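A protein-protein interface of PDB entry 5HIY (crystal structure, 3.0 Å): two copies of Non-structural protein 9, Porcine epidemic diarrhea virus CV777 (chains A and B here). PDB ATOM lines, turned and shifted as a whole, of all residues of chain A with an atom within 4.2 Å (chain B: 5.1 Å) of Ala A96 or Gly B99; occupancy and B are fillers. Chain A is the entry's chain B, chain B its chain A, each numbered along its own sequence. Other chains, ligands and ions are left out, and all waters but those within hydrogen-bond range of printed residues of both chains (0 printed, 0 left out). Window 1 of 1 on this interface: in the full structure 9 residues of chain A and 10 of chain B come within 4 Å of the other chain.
The backbone NH (N) of Ala A96 sits close to the backbone carbonyl oxygen (O) of Gly B95 (3.1 Å). The backbone NH (N) of Ala B96 sits close to the backbone carbonyl oxygen (O) of Gly A95.
O of Leu A92 touches CA of Gly B95, at 3.6 Å. Gly B95 touches Gly A95. Ala A96 touches Ala B96. CA of Gly B99 touches O of Ala A96 (3.6 Å). Ala B96 touches Gly A99 (O to CA, 3.6 Å). C of Gly A99 touches C of Gly B99, at 3.8 Å. Tyr B100 touches Gly A99. Tyr A100 touches Gly B99. CB of Ala B103 touches CD2 of Tyr A100 (3.9 Å).
Of chain B, only Gly B95, Ala B96 and Gly B99 come within 4 Å of Ala A96. Printed residues of chain B within 4 Å of Tyr A100: Gly B99 (3.7 Å) and Ala B103 (3.9 Å). Printed residues of chain A within 4 Å of Gly B95: Leu A92 (3.6 Å), Gly A95 (3.3 Å) and Ala A96 (3.0 Å). Gly B99 touches just these residues of chain A: Ala A96, Gly A99 and Tyr A100.
Of the 9 printed residues of chain A, 5 touch a printed residue of chain B. Of the 10 printed residues of chain B, 5 touch a printed residue of chain A. Hydrophobic or aromatic side chains of chain B that line the printed part of chain A: Ala B96 and Ala B103. Among the printed residues, 11 pairs touch across the chains.
Gly B95 touches its own counterpart, Gly A95. Gly A95 touches Ala B96, and with the chains exchanged Ala A96 touches Gly B95. Ala A96 touches its own counterpart, Ala B96. Gly A99 touches Tyr B100, and with the chains exchanged Tyr A100 touches Gly B99. Of the 11 pairs that touch across the chains among the printed residues, 9 have their exchanged pair printed and touching as well.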
ATOM      1  N   LEU A  92       1.835  13.575  13.358  1.00  0.00           N
ATOM      2  CA  LEU A  92       3.212  13.955  13.619  1.00  0.00           C
ATOM      3  C   LEU A  92       3.623  14.907  12.517  1.00  0.00           C
ATOM      4  O   LEU A  92       3.696  16.116  12.724  1.00  0.00           O
ATOM      5  CB  LEU A  92       4.149  12.744  13.658  1.00  0.00           C
ATOM      6  CG  LEU A  92       5.551  13.024  14.235  1.00  0.00           C
ATOM      7  CD1 LEU A  92       5.539  12.973  15.744  1.00  0.00           C
ATOM      8  CD2 LEU A  92       6.601  12.065  13.686  1.00  0.00           C
ATOM      9  N   ARG A  93       3.853  14.354  11.332  1.00  0.00           N
ATOM     10  CA  ARG A  93       4.185  15.143  10.146  1.00  0.00           C
ATOM     11  C   ARG A  93       3.281  16.382   9.915  1.00  0.00           C
ATOM     12  O   ARG A  93       3.666  17.279   9.177  1.00  0.00           O
ATOM     13  CB  ARG A  93       4.171  14.238   8.912  1.00  0.00           C
ATOM     14  CG  ARG A  93       5.127  13.065   8.977  1.00  0.00           C
ATOM     15  CD  ARG A  93       5.281  12.485   7.598  1.00  0.00           C
ATOM     16  NE  ARG A  93       6.540  11.778   7.384  1.00  0.00           N
ATOM     17  CZ  ARG A  93       6.635  10.460   7.205  1.00  0.00           C
ATOM     18  NH1 ARG A  93       7.827   9.901   7.005  1.00  0.00           N
ATOM     19  NH2 ARG A  93       5.541   9.699   7.230  1.00  0.00           N
ATOM     20  N   ARG A  94       2.091  16.420  10.520  1.00  0.00           N
ATOM     21  CA  ARG A  94       1.228  17.596  10.432  1.00  0.00           C
ATOM     22  C   ARG A  94       1.789  18.719  11.277  1.00  0.00           C
ATOM     23  O   ARG A  94       1.681  19.896  10.922  1.00  0.00           O
ATOM     24  CB  ARG A  94      -0.195  17.290  10.913  1.00  0.00           C
ATOM     25  CG  ARG A  94      -1.189  16.931   9.826  1.00  0.00           C
ATOM     26  CD  ARG A  94      -2.488  16.398  10.417  1.00  0.00           C
ATOM     27  NE  ARG A  94      -3.628  16.914   9.668  1.00  0.00           N
ATOM     28  CZ  ARG A  94      -4.276  16.270   8.697  1.00  0.00           C
ATOM     29  NH1 ARG A  94      -3.952  15.034   8.332  1.00  0.00           N
ATOM     30  NH2 ARG A  94      -5.280  16.882   8.089  1.00  0.00           N
ATOM     31  N   GLY A  95       2.372  18.342  12.406  1.00  0.00           N
ATOM     32  CA  GLY A  95       2.947  19.285  13.355  1.00  0.00           C
ATOM     33  C   GLY A  95       4.151  20.012  12.799  1.00  0.00           C
ATOM     34  O   GLY A  95       4.274  21.216  12.985  1.00  0.00           O
ATOM     35  N   ALA A  96       5.037  19.291  12.115  1.00  0.00           N
ATOM     36  CA  ALA A  96       6.207  19.921  11.493  1.00  0.00           C
ATOM     37  C   ALA A  96       5.820  20.939  10.423  1.00  0.00           C
ATOM     38  O   ALA A  96       6.309  22.070  10.444  1.00  0.00           O
ATOM     39  CB  ALA A  96       7.142  18.889  10.928  1.00  0.00           C
ATOM     40  N   VAL A  97       4.930  20.551   9.512  1.00  0.00           N
ATOM     41  CA  VAL A  97       4.374  21.500   8.562  1.00  0.00           C
ATOM     42  C   VAL A  97       4.031  22.797   9.287  1.00  0.00           C
ATOM     43  O   VAL A  97       4.402  23.880   8.846  1.00  0.00           O
ATOM     44  CB  VAL A  97       3.118  20.942   7.848  1.00  0.00           C
ATOM     45  CG1 VAL A  97       2.366  22.050   7.102  1.00  0.00           C
ATOM     46  CG2 VAL A  97       3.504  19.842   6.878  1.00  0.00           C
ATOM     47  N   LEU A  98       3.348  22.680  10.416  1.00  0.00           N
ATOM     48  CA  LEU A  98       2.873  23.853  11.116  1.00  0.00           C
ATOM     49  C   LEU A  98       3.967  24.560  11.892  1.00  0.00           C
ATOM     50  O   LEU A  98       3.939  25.784  12.039  1.00  0.00           O
ATOM     51  CB  LEU A  98       1.723  23.492  12.038  1.00  0.00           C
ATOM     52  CG  LEU A  98       0.389  23.293  11.322  1.00  0.00           C
ATOM     53  CD1 LEU A  98      -0.600  22.666  12.277  1.00  0.00           C
ATOM     54  CD2 LEU A  98      -0.146  24.626  10.767  1.00  0.00           C
ATOM     55  N   GLY A  99       4.932  23.793  12.383  1.00  0.00           N
ATOM     56  CA  GLY A  99       6.013  24.359  13.172  1.00  0.00           C
ATOM     57  C   GLY A  99       7.010  25.006  12.244  1.00  0.00           C
ATOM     58  O   GLY A  99       7.716  25.938  12.624  1.00  0.00           O
ATOM     59  N   TYR A 100       7.066  24.505  11.015  1.00  0.00           N
ATOM     60  CA  TYR A 100       8.000  24.994  10.027  1.00  0.00           C
ATOM     61  C   TYR A 100       7.517  26.362   9.554  1.00  0.00           C
ATOM     62  O   TYR A 100       8.185  27.382   9.748  1.00  0.00           O
ATOM     63  CB  TYR A 100       8.068  23.996   8.872  1.00  0.00           C
ATOM     64  CG  TYR A 100       8.904  24.447   7.718  1.00  0.00           C
ATOM     65  CD1 TYR A 100       8.344  25.158   6.666  1.00  0.00           C
ATOM     66  CD2 TYR A 100      10.260  24.160   7.673  1.00  0.00           C
ATOM     67  CE1 TYR A 100       9.116  25.574   5.602  1.00  0.00           C
ATOM     68  CE2 TYR A 100      11.043  24.573   6.614  1.00  0.00           C
ATOM     69  CZ  TYR A 100      10.468  25.281   5.585  1.00  0.00           C
ATOM     70  OH  TYR A 100      11.251  25.691   4.540  1.00  0.00           O
ATOM     71  N   ARG B  94       4.800  17.651  19.106  1.00  0.00           N
ATOM     72  CA  ARG B  94       6.114  17.062  18.864  1.00  0.00           C
ATOM     73  C   ARG B  94       6.597  17.348  17.443  1.00  0.00           C
ATOM     74  O   ARG B  94       7.727  17.800  17.230  1.00  0.00           O
ATOM     75  CB  ARG B  94       6.080  15.548  19.107  1.00  0.00           C
ATOM     76  CG  ARG B  94       6.214  15.123  20.571  1.00  0.00           C
ATOM     77  CD  ARG B  94       5.647  13.715  20.814  1.00  0.00           C
ATOM     78  NE  ARG B  94       6.515  12.954  21.708  1.00  0.00           N
ATOM     79  CZ  ARG B  94       6.345  12.828  23.023  1.00  0.00           C
ATOM     80  NH1 ARG B  94       5.316  13.391  23.641  1.00  0.00           N
ATOM     81  NH2 ARG B  94       7.224  12.131  23.730  1.00  0.00           N
ATOM     82  N   GLY B  95       5.739  17.068  16.467  1.00  0.00           N
ATOM     83  CA  GLY B  95       6.026  17.405  15.079  1.00  0.00           C
ATOM     84  C   GLY B  95       6.293  18.889  14.979  1.00  0.00           C
ATOM     85  O   GLY B  95       7.205  19.309  14.278  1.00  0.00           O
ATOM     86  N   ALA B  96       5.506  19.677  15.710  1.00  0.00           N
ATOM     87  CA  ALA B  96       5.685  21.125  15.760  1.00  0.00           C
ATOM     88  C   ALA B  96       7.065  21.520  16.242  1.00  0.00           C
ATOM     89  O   ALA B  96       7.637  22.498  15.756  1.00  0.00           O
ATOM     90  CB  ALA B  96       4.645  21.763  16.625  1.00  0.00           C
ATOM     91  N   VAL B  97       7.605  20.764  17.189  1.00  0.00           N
ATOM     92  CA  VAL B  97       8.925  21.067  17.686  1.00  0.00           C
ATOM     93  C   VAL B  97       9.935  20.765  16.594  1.00  0.00           C
ATOM     94  O   VAL B  97      10.789  21.593  16.284  1.00  0.00           O
ATOM     95  CB  VAL B  97       9.241  20.289  18.962  1.00  0.00           C
ATOM     96  CG1 VAL B  97      10.740  20.327  19.269  1.00  0.00           C
ATOM     97  CG2 VAL B  97       8.426  20.835  20.125  1.00  0.00           C
ATOM     98  N   LEU B  98       9.808  19.600  15.977  1.00  0.00           N
ATOM     99  CA  LEU B  98      10.768  19.173  14.964  1.00  0.00           C
ATOM    100  C   LEU B  98      10.664  20.039  13.717  1.00  0.00           C
ATOM    101  O   LEU B  98      11.609  20.146  12.941  1.00  0.00           O
ATOM    102  CB  LEU B  98      10.557  17.699  14.627  1.00  0.00           C
ATOM    103  CG  LEU B  98      10.521  16.731  15.822  1.00  0.00           C
ATOM    104  CD1 LEU B  98       9.650  15.534  15.528  1.00  0.00           C
ATOM    105  CD2 LEU B  98      11.916  16.287  16.235  1.00  0.00           C
ATOM    106  N   GLY B  99       9.508  20.670  13.541  1.00  0.00           N
ATOM    107  CA  GLY B  99       9.297  21.616  12.443  1.00  0.00           C
ATOM    108  C   GLY B  99      10.164  22.855  12.585  1.00  0.00           C
ATOM    109  O   GLY B  99      10.819  23.281  11.629  1.00  0.00           O
ATOM    110  N   TYR B 100      10.163  23.414  13.793  1.00  0.00           N
ATOM    111  CA  TYR B 100      10.966  24.584  14.161  1.00  0.00           C
ATOM    112  C   TYR B 100      12.466  24.328  13.991  1.00  0.00           C
ATOM    113  O   TYR B 100      13.136  25.035  13.232  1.00  0.00           O
ATOM    114  CB  TYR B 100      10.643  24.948  15.607  1.00  0.00           C
ATOM    115  CG  TYR B 100      11.310  26.174  16.166  1.00  0.00           C
ATOM    116  CD1 TYR B 100      12.533  26.072  16.834  1.00  0.00           C
ATOM    117  CD2 TYR B 100      10.696  27.427  16.091  1.00  0.00           C
ATOM    118  CE1 TYR B 100      13.147  27.193  17.389  1.00  0.00           C
ATOM    119  CE2 TYR B 100      11.299  28.556  16.644  1.00  0.00           C
ATOM    120  CZ  TYR B 100      12.526  28.426  17.292  1.00  0.00           C
ATOM    121  OH  TYR B 100      13.154  29.520  17.845  1.00  0.00           O
ATOM    122  N   ILE B 101      12.981  23.313  14.684  1.00  0.00           N
ATOM    123  CA  ILE B 101      14.407  22.997  14.631  1.00  0.00           C
ATOM    124  C   ILE B 101      14.874  22.856  13.184  1.00  0.00           C
ATOM    125  O   ILE B 101      15.716  23.629  12.723  1.00  0.00           O
ATOM    126  CB  ILE B 101      14.778  21.695  15.395  1.00  0.00           C
ATOM    127  CG1 ILE B 101      13.896  21.471  16.635  1.00  0.00           C
ATOM    128  CG2 ILE B 101      16.265  21.687  15.739  1.00  0.00           C
ATOM    129  CD1 ILE B 101      13.807  22.631  17.606  1.00  0.00           C
ATOM    130  N   GLY B 102      14.302  21.880  12.474  1.00  0.00           N
ATOM    131  CA  GLY B 102      14.661  21.584  11.081  1.00  0.00           C
ATOM    132  C   GLY B 102      14.324  22.699  10.105  1.00  0.00           C
ATOM    133  O   GLY B 102      14.104  22.446   8.915  1.00  0.00           O
ATOM    134  N   ALA B 103      14.249  23.921  10.633  1.00  0.00           N
ATOM    135  CA  ALA B 103      14.200  25.150   9.844  1.00  0.00           C
ATOM    136  C   ALA B 103      15.361  26.036  10.278  1.00  0.00           C
ATOM    137  O   ALA B 103      16.017  26.666   9.442  1.00  0.00           O
ATOM    138  CB  ALA B 103      12.873  25.878  10.037  1.00  0.00           C
